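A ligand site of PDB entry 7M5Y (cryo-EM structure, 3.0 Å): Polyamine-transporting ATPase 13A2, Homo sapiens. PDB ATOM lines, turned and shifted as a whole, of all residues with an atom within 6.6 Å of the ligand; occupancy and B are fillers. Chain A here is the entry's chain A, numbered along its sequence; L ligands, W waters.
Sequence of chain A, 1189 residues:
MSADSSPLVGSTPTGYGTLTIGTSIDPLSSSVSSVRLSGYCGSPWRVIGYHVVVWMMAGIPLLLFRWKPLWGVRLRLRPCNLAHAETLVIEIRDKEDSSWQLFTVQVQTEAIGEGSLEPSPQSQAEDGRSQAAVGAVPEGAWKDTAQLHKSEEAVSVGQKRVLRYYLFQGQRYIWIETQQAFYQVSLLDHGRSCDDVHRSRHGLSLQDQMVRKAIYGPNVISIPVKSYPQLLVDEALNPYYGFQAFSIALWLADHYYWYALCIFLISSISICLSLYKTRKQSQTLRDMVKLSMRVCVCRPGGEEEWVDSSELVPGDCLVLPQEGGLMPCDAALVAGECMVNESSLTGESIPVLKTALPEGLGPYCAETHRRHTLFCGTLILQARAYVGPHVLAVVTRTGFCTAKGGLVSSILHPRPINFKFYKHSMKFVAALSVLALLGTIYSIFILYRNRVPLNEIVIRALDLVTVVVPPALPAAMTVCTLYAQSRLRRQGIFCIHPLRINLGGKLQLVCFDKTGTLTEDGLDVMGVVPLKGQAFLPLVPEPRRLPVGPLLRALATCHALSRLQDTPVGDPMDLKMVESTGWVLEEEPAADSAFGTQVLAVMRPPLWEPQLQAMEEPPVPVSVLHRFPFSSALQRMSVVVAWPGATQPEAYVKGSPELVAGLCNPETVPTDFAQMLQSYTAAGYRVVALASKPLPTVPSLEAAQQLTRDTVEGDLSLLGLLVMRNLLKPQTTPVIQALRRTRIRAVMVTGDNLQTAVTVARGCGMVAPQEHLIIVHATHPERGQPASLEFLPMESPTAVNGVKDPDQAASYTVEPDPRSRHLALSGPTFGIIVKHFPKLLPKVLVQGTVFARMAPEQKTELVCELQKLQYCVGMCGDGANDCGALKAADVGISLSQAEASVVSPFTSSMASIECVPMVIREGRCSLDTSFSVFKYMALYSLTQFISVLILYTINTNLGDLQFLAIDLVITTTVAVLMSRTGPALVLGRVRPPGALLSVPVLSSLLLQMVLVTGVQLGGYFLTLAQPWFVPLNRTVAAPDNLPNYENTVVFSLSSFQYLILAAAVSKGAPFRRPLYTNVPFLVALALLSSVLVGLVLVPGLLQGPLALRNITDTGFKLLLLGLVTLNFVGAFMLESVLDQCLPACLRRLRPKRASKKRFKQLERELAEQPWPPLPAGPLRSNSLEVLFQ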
ATOM      1  N   TRP A 251     -10.008  25.096   3.874  1.00  0.00           N
ATOM      2  CA  TRP A 251      -9.002  24.510   3.002  1.00  0.00           C
ATOM      3  C   TRP A 251      -8.404  25.558   2.069  1.00  0.00           C
ATOM      4  O   TRP A 251      -7.194  25.546   1.794  1.00  0.00           O
ATOM      5  CB  TRP A 251      -9.619  23.365   2.198  1.00  0.00           C
ATOM      6  CG  TRP A 251      -9.899  22.107   2.997  1.00  0.00           C
ATOM      7  CD1 TRP A 251      -9.324  21.735   4.185  1.00  0.00           C
ATOM      8  CD2 TRP A 251     -10.830  21.083   2.667  1.00  0.00           C
ATOM      9  NE1 TRP A 251      -9.837  20.533   4.601  1.00  0.00           N
ATOM     10  CE2 TRP A 251     -10.768  20.107   3.691  1.00  0.00           C
ATOM     11  CE3 TRP A 251     -11.717  20.885   1.607  1.00  0.00           C
ATOM     12  CZ2 TRP A 251     -11.552  18.961   3.685  1.00  0.00           C
ATOM     13  CZ3 TRP A 251     -12.502  19.748   1.606  1.00  0.00           C
ATOM     14  CH2 TRP A 251     -12.410  18.800   2.633  1.00  0.00           C
ATOM     15  N   ASP A 254      -5.916  27.202   3.890  1.00  0.00           N
ATOM     16  CA  ASP A 254      -4.747  26.367   4.166  1.00  0.00           C
ATOM     17  C   ASP A 254      -4.070  25.876   2.887  1.00  0.00           C
ATOM     18  O   ASP A 254      -3.312  24.893   2.921  1.00  0.00           O
ATOM     19  CB  ASP A 254      -5.163  25.179   5.043  1.00  0.00           C
ATOM     20  CG  ASP A 254      -3.993  24.518   5.746  1.00  0.00           C
ATOM     21  OD1 ASP A 254      -2.842  24.940   5.542  1.00  0.00           O
ATOM     22  OD2 ASP A 254      -4.232  23.572   6.517  1.00  0.00           O
ATOM     23  N   HIS A 255      -4.323  26.517   1.749  1.00  0.00           N
ATOM     24  CA  HIS A 255      -3.633  26.214   0.490  1.00  0.00           C
ATOM     25  C   HIS A 255      -3.941  24.800  -0.020  1.00  0.00           C
ATOM     26  O   HIS A 255      -3.206  24.265  -0.851  1.00  0.00           O
ATOM     27  CB  HIS A 255      -2.119  26.412   0.603  1.00  0.00           C
ATOM     28  CG  HIS A 255      -1.711  27.762   1.075  1.00  0.00           C
ATOM     29  ND1 HIS A 255      -1.981  28.222   2.350  1.00  0.00           N
ATOM     30  CD2 HIS A 255      -1.065  28.773   0.444  1.00  0.00           C
ATOM     31  CE1 HIS A 255      -1.508  29.449   2.475  1.00  0.00           C
ATOM     32  NE2 HIS A 255      -0.950  29.804   1.337  1.00  0.00           N
ATOM     33  N   TYR A 256      -5.025  24.195   0.465  1.00  0.00           N
ATOM     34  CA  TYR A 256      -5.468  22.879   0.001  1.00  0.00           C
ATOM     35  C   TYR A 256      -6.569  23.097  -1.032  1.00  0.00           C
ATOM     36  O   TYR A 256      -7.750  22.830  -0.806  1.00  0.00           O
ATOM     37  CB  TYR A 256      -5.928  22.031   1.193  1.00  0.00           C
ATOM     38  CG  TYR A 256      -5.946  20.524   0.966  1.00  0.00           C
ATOM     39  CD1 TYR A 256      -4.832  19.848   0.496  1.00  0.00           C
ATOM     40  CD2 TYR A 256      -7.083  19.785   1.251  1.00  0.00           C
ATOM     41  CE1 TYR A 256      -4.850  18.488   0.297  1.00  0.00           C
ATOM     42  CE2 TYR A 256      -7.113  18.419   1.056  1.00  0.00           C
ATOM     43  CZ  TYR A 256      -5.999  17.779   0.584  1.00  0.00           C
ATOM     44  OH  TYR A 256      -6.020  16.414   0.393  1.00  0.00           O
ATOM     45  N   TYR A 259      -8.689  19.608  -3.317  1.00  0.00           N
ATOM     46  CA  TYR A 259      -9.778  18.862  -2.700  1.00  0.00           C
ATOM     47  C   TYR A 259     -10.958  19.765  -2.398  1.00  0.00           C
ATOM     48  O   TYR A 259     -12.111  19.344  -2.477  1.00  0.00           O
ATOM     49  CB  TYR A 259      -9.319  18.156  -1.427  1.00  0.00           C
ATOM     50  CG  TYR A 259     -10.201  17.007  -0.992  1.00  0.00           C
ATOM     51  CD1 TYR A 259     -10.443  15.921  -1.830  1.00  0.00           C
ATOM     52  CD2 TYR A 259     -10.801  16.999   0.257  1.00  0.00           C
ATOM     53  CE1 TYR A 259     -11.256  14.879  -1.439  1.00  0.00           C
ATOM     54  CE2 TYR A 259     -11.610  15.961   0.664  1.00  0.00           C
ATOM     55  CZ  TYR A 259     -11.834  14.899  -0.190  1.00  0.00           C
ATOM     56  OH  TYR A 259     -12.638  13.857   0.204  1.00  0.00           O
ATOM     57  N   GLU A 456      -0.971  29.747  12.385  1.00  0.00           N
ATOM     58  CA  GLU A 456      -0.754  28.342  12.098  1.00  0.00           C
ATOM     59  C   GLU A 456      -1.452  27.445  13.099  1.00  0.00           C
ATOM     60  O   GLU A 456      -2.044  26.435  12.718  1.00  0.00           O
ATOM     61  CB  GLU A 456       0.746  28.032  12.079  1.00  0.00           C
ATOM     62  CG  GLU A 456       1.506  28.705  10.940  1.00  0.00           C
ATOM     63  CD  GLU A 456       2.640  27.845  10.389  1.00  0.00           C
ATOM     64  OE1 GLU A 456       2.431  26.633  10.186  1.00  0.00           O
ATOM     65  OE2 GLU A 456       3.736  28.397  10.159  1.00  0.00           O
ATOM     66  N   ARG A 460      -4.300  24.758  12.055  1.00  0.00           N
ATOM     67  CA  ARG A 460      -4.070  23.330  12.311  1.00  0.00           C
ATOM     68  C   ARG A 460      -5.172  22.761  13.192  1.00  0.00           C
ATOM     69  O   ARG A 460      -5.689  21.671  12.926  1.00  0.00           O
ATOM     70  CB  ARG A 460      -2.703  23.124  12.971  1.00  0.00           C
ATOM     71  CG  ARG A 460      -1.500  23.592  12.164  1.00  0.00           C
ATOM     72  CD  ARG A 460      -0.841  22.464  11.398  1.00  0.00           C
ATOM     73  NE  ARG A 460      -1.738  21.888  10.397  1.00  0.00           N
ATOM     74  CZ  ARG A 460      -2.077  22.486   9.262  1.00  0.00           C
ATOM     75  NH1 ARG A 460      -1.605  23.683   8.927  1.00  0.00           N
ATOM     76  NH2 ARG A 460      -2.918  21.866   8.427  1.00  0.00           N
ATOM     77  N   ASP A 463      -8.389  22.348  11.167  1.00  0.00           N
ATOM     78  CA  ASP A 463      -8.381  21.280  10.174  1.00  0.00           C
ATOM     79  C   ASP A 463      -8.611  19.888  10.749  1.00  0.00           C
ATOM     80  O   ASP A 463      -9.130  19.018  10.027  1.00  0.00           O
ATOM     81  CB  ASP A 463      -7.047  21.296   9.421  1.00  0.00           C
ATOM     82  CG  ASP A 463      -6.942  20.197   8.395  1.00  0.00           C
ATOM     83  OD1 ASP A 463      -7.892  20.005   7.622  1.00  0.00           O
ATOM     84  OD2 ASP A 463      -5.894  19.514   8.364  1.00  0.00           O
ATOM     85  N   THR A 466     -12.333  18.817  10.360  1.00  0.00           N
ATOM     86  CA  THR A 466     -12.661  18.324   9.029  1.00  0.00           C
ATOM     87  C   THR A 466     -12.033  16.958   8.782  1.00  0.00           C
ATOM     88  O   THR A 466     -12.605  16.137   8.057  1.00  0.00           O
ATOM     89  CB  THR A 466     -12.203  19.305   7.954  1.00  0.00           C
ATOM     90  OG1 THR A 466     -10.771  19.421   7.974  1.00  0.00           O
ATOM     91  CG2 THR A 466     -12.825  20.681   8.185  1.00  0.00           C
ATOM     92  N   VAL A 467     -10.860  16.699   9.362  1.00  0.00           N
ATOM     93  CA  VAL A 467     -10.283  15.358   9.283  1.00  0.00           C
ATOM     94  C   VAL A 467     -11.189  14.352   9.981  1.00  0.00           C
ATOM     95  O   VAL A 467     -11.376  13.231   9.486  1.00  0.00           O
ATOM     96  CB  VAL A 467      -8.857  15.355   9.867  1.00  0.00           C
ATOM     97  CG1 VAL A 467      -8.352  13.924  10.038  1.00  0.00           C
ATOM     98  CG2 VAL A 467      -7.912  16.140   8.975  1.00  0.00           C
ATOM     99  N   PRO A 471     -16.242  15.654   4.951  1.00  0.00           N
ATOM    100  CA  PRO A 471     -17.222  16.429   4.192  1.00  0.00           C
ATOM    101  C   PRO A 471     -17.704  15.727   2.935  1.00  0.00           C
ATOM    102  O   PRO A 471     -18.672  16.186   2.319  1.00  0.00           O
ATOM    103  CB  PRO A 471     -16.471  17.732   3.852  1.00  0.00           C
ATOM    104  CG  PRO A 471     -15.309  17.758   4.774  1.00  0.00           C
ATOM    105  CD  PRO A 471     -14.933  16.333   4.951  1.00  0.00           C
ATOM    106  N   TYR A 940     -11.712   5.418   7.401  1.00  0.00           N
ATOM    107  CA  TYR A 940     -10.900   6.372   6.637  1.00  0.00           C
ATOM    108  C   TYR A 940     -10.645   7.631   7.438  1.00  0.00           C
ATOM    109  O   TYR A 940      -9.503   8.074   7.576  1.00  0.00           O
ATOM    110  CB  TYR A 940     -11.533   6.702   5.291  1.00  0.00           C
ATOM    111  CG  TYR A 940     -11.195   8.091   4.827  1.00  0.00           C
ATOM    112  CD1 TYR A 940      -9.955   8.377   4.267  1.00  0.00           C
ATOM    113  CD2 TYR A 940     -12.124   9.128   4.910  1.00  0.00           C
ATOM    114  CE1 TYR A 940      -9.630   9.652   3.839  1.00  0.00           C
ATOM    115  CE2 TYR A 940     -11.809  10.403   4.478  1.00  0.00           C
ATOM    116  CZ  TYR A 940     -10.574  10.656   3.933  1.00  0.00           C
ATOM    117  OH  TYR A 940     -10.261  11.926   3.510  1.00  0.00           O
ATOM    118  N   GLN A 944      -6.961   8.325   9.782  1.00  0.00           N
ATOM    119  CA  GLN A 944      -6.250   9.519   9.348  1.00  0.00           C
ATOM    120  C   GLN A 944      -6.057  10.460  10.522  1.00  0.00           C
ATOM    121  O   GLN A 944      -4.941  10.924  10.786  1.00  0.00           O
ATOM    122  CB  GLN A 944      -7.021  10.219   8.227  1.00  0.00           C
ATOM    123  CG  GLN A 944      -6.207  11.245   7.459  1.00  0.00           C
ATOM    124  CD  GLN A 944      -7.012  11.920   6.371  1.00  0.00           C
ATOM    125  OE1 GLN A 944      -8.203  11.669   6.222  1.00  0.00           O
ATOM    126  NE2 GLN A 944      -6.358  12.786   5.605  1.00  0.00           N
ATOM    127  N   TYR A 952       1.414  15.386  14.671  1.00  0.00           N
ATOM    128  CA  TYR A 952       1.250  16.633  15.421  1.00  0.00           C
ATOM    129  C   TYR A 952       1.918  16.540  16.789  1.00  0.00           C
ATOM    130  O   TYR A 952       2.251  17.569  17.381  1.00  0.00           O
ATOM    131  CB  TYR A 952      -0.234  16.953  15.599  1.00  0.00           C
ATOM    132  CG  TYR A 952      -0.885  17.728  14.470  1.00  0.00           C
ATOM    133  CD1 TYR A 952      -0.424  17.646  13.164  1.00  0.00           C
ATOM    134  CD2 TYR A 952      -1.982  18.537  14.720  1.00  0.00           C
ATOM    135  CE1 TYR A 952      -1.028  18.363  12.140  1.00  0.00           C
ATOM    136  CE2 TYR A 952      -2.591  19.258  13.708  1.00  0.00           C
ATOM    137  CZ  TYR A 952      -2.115  19.157  12.421  1.00  0.00           C
ATOM    138  OH  TYR A 952      -2.726  19.864  11.413  1.00  0.00           O
ATOM    139  N   ASN A 957       3.389  17.187   9.975  1.00  0.00           N
ATOM    140  CA  ASN A 957       2.121  16.965   9.312  1.00  0.00           C
ATOM    141  C   ASN A 957       2.381  16.052   8.125  1.00  0.00           C
ATOM    142  O   ASN A 957       3.538  15.847   7.738  1.00  0.00           O
ATOM    143  CB  ASN A 957       1.486  18.299   8.886  1.00  0.00           C
ATOM    144  CG  ASN A 957       0.031  18.157   8.497  1.00  0.00           C
ATOM    145  OD1 ASN A 957      -0.670  17.261   8.958  1.00  0.00           O
ATOM    146  ND2 ASN A 957      -0.435  19.074   7.646  1.00  0.00           N
ATOM    147  N   GLY A 959       1.478  16.274   4.711  1.00  0.00           N
ATOM    148  CA  GLY A 959       1.944  16.935   3.504  1.00  0.00           C
ATOM    149  C   GLY A 959       0.835  17.093   2.493  1.00  0.00           C
ATOM    150  O   GLY A 959      -0.086  16.273   2.452  1.00  0.00           O
ATOM    151  N   ASP A 960       0.898  18.154   1.679  1.00  0.00           N
ATOM    152  CA  ASP A 960      -0.188  18.434   0.750  1.00  0.00           C
ATOM    153  C   ASP A 960      -0.371  17.295  -0.246  1.00  0.00           C
ATOM    154  O   ASP A 960      -1.494  16.844  -0.493  1.00  0.00           O
ATOM    155  CB  ASP A 960       0.079  19.746   0.017  1.00  0.00           C
ATOM    156  CG  ASP A 960       0.057  20.956   0.932  1.00  0.00           C
ATOM    157  OD1 ASP A 960      -0.839  21.025   1.799  1.00  0.00           O
ATOM    158  OD2 ASP A 960       0.945  21.816   0.801  1.00  0.00           O
ATOM    159  N   PHE A 963      -1.681  14.265   1.621  1.00  0.00           N
ATOM    160  CA  PHE A 963      -3.092  14.462   1.948  1.00  0.00           C
ATOM    161  C   PHE A 963      -3.957  14.248   0.713  1.00  0.00           C
ATOM    162  O   PHE A 963      -5.027  13.625   0.786  1.00  0.00           O
ATOM    163  CB  PHE A 963      -3.335  15.865   2.507  1.00  0.00           C
ATOM    164  CG  PHE A 963      -3.318  15.934   4.017  1.00  0.00           C
ATOM    165  CD1 PHE A 963      -4.246  15.260   4.774  1.00  0.00           C
ATOM    166  CD2 PHE A 963      -2.367  16.710   4.668  1.00  0.00           C
ATOM    167  CE1 PHE A 963      -4.232  15.331   6.149  1.00  0.00           C
ATOM    168  CE2 PHE A 963      -2.351  16.795   6.040  1.00  0.00           C
ATOM    169  CZ  PHE A 963      -3.286  16.103   6.785  1.00  0.00           C
ATOM    170  N   ASP A 967      -6.890  11.561   0.044  1.00  0.00           N
ATOM    171  CA  ASP A 967      -8.279  11.975  -0.067  1.00  0.00           C
ATOM    172  C   ASP A 967      -8.860  11.767  -1.464  1.00  0.00           C
ATOM    173  O   ASP A 967     -10.018  11.380  -1.586  1.00  0.00           O
ATOM    174  CB  ASP A 967      -8.403  13.447   0.344  1.00  0.00           C
ATOM    175  CG  ASP A 967      -7.949  13.696   1.769  1.00  0.00           C
ATOM    176  OD1 ASP A 967      -8.047  12.764   2.588  1.00  0.00           O
ATOM    177  OD2 ASP A 967      -7.508  14.823   2.067  1.00  0.00           O
ATOM    178  N   PRO A1039       5.360  21.670   7.752  1.00  0.00           N
ATOM    179  CA  PRO A1039       5.597  21.265   6.364  1.00  0.00           C
ATOM    180  C   PRO A1039       7.042  21.370   5.915  1.00  0.00           C
ATOM    181  O   PRO A1039       7.437  20.652   4.996  1.00  0.00           O
ATOM    182  CB  PRO A1039       4.705  22.227   5.567  1.00  0.00           C
ATOM    183  CG  PRO A1039       4.664  23.437   6.390  1.00  0.00           C
ATOM    184  CD  PRO A1039       4.693  22.978   7.815  1.00  0.00           C
HETATM  185  N1  LIG L   1      -8.825  15.214   4.818  1.00  0.00           N
HETATM  186  C1  LIG L   1      -8.903  16.708   4.990  1.00  0.00           C
HETATM  187  C2  LIG L   1      -7.586  17.184   5.605  1.00  0.00           C
HETATM  188  C3  LIG L   1      -6.826  18.084   4.666  1.00  0.00           C
HETATM  189  N2  LIG L   1      -5.657  18.690   5.393  1.00  0.00           N
HETATM  190  C4  LIG L   1      -4.824  19.416   4.374  1.00  0.00           C
HETATM  191  C5  LIG L   1      -3.791  20.172   5.179  1.00  0.00           C
HETATM  192  C6  LIG L   1      -2.889  20.793   4.146  1.00  0.00           C
HETATM  193  C7  LIG L   1      -1.857  21.520   4.982  1.00  0.00           C
HETATM  194  N3  LIG L   1      -1.031  22.281   3.982  1.00  0.00           N
HETATM  195  C8  LIG L   1      -0.094  23.199   4.728  1.00  0.00           C
HETATM  196  C9  LIG L   1       0.467  24.136   3.664  1.00  0.00           C
HETATM  197  C10 LIG L   1       1.320  25.171   4.377  1.00  0.00           C
HETATM  198  N4  LIG L   1       1.524  26.349   3.440  1.00  0.00           N
HETATM  199  O   HOH W   1       1.206  20.069   5.677  1.00  0.00           O
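The side-chain carboxylate (OD2) of Asp 463 is in salt-bridge range of a nitrogen (N2) of the ligand, at 3.1 Å.
OD1 of Asp 254 lies within salt-bridge range of N3 of the ligand, 3.6 Å away.
A nitrogen (N1) of the ligand is in salt-bridge range of the side-chain carboxylate (OD2) of Asp 967 (3.1 Å).
OD1 of Asp 960 is in salt-bridge range of N3 of the ligand, at 2.5 Å.
The guanidinium group (NH2) of Arg 460 lies within salt-bridge range of the side-chain carboxylate (OD2) of Asp 463, 3.8 Å away.
The side-chain hydroxyl (OH) of Tyr 940 is in hydrogen-bond range of the side-chain amide oxygen (OE1) of Gln 944.
The side-chain carboxylate (OD1) of Asp 967 sits at hydrogen-bond distance from the side-chain amide nitrogen (NE2) of Gln 944 (3.5 Å).
The backbone carbonyl oxygen (O) of Phe 963 sits at hydrogen-bond distance from the side-chain hydroxyl (OH) of Tyr 256, at 3.0 Å.
The backbone carbonyl oxygen (O) of Trp 251 is in hydrogen-bond range of the backbone NH (N) of Tyr 256 (2.9 Å).
O of Asp 463 is in hydrogen-bond range of OG1 of Thr 466 (2.7 Å).
The side-chain carboxylate (OD2) of Asp 254 is in salt-bridge range of the guanidinium group (NH2) of Arg 460, 2.9 Å away.
OH of Tyr 952 is in hydrogen-bond range of NE of Arg 460 (2.5 Å).
Residues that only touch the ligand: Trp 251 (3.7 Å), Tyr 256 (3.6 Å), Arg 460 (3.6 Å), Val 467 (3.5 Å), Tyr 940 (3.8 Å), Gln 944 (3.5 Å), Asn 957 (3.9 Å) and Phe 963 (3.7 Å).
Hydrophobic or aromatic side chains that line the ligand: Trp 251, Tyr 256, Val 467 and Phe 963.
12 residues have an atom within 4 Å of the ligand: Trp 251, Asp 254, Tyr 256, Arg 460, Asp 463, Val 467, Tyr 940, Gln 944, Asn 957, Asp 960, Phe 963 and Asp 967.
The nearest printed residue that does not touch the ligand is His 255 (4.1 Å).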
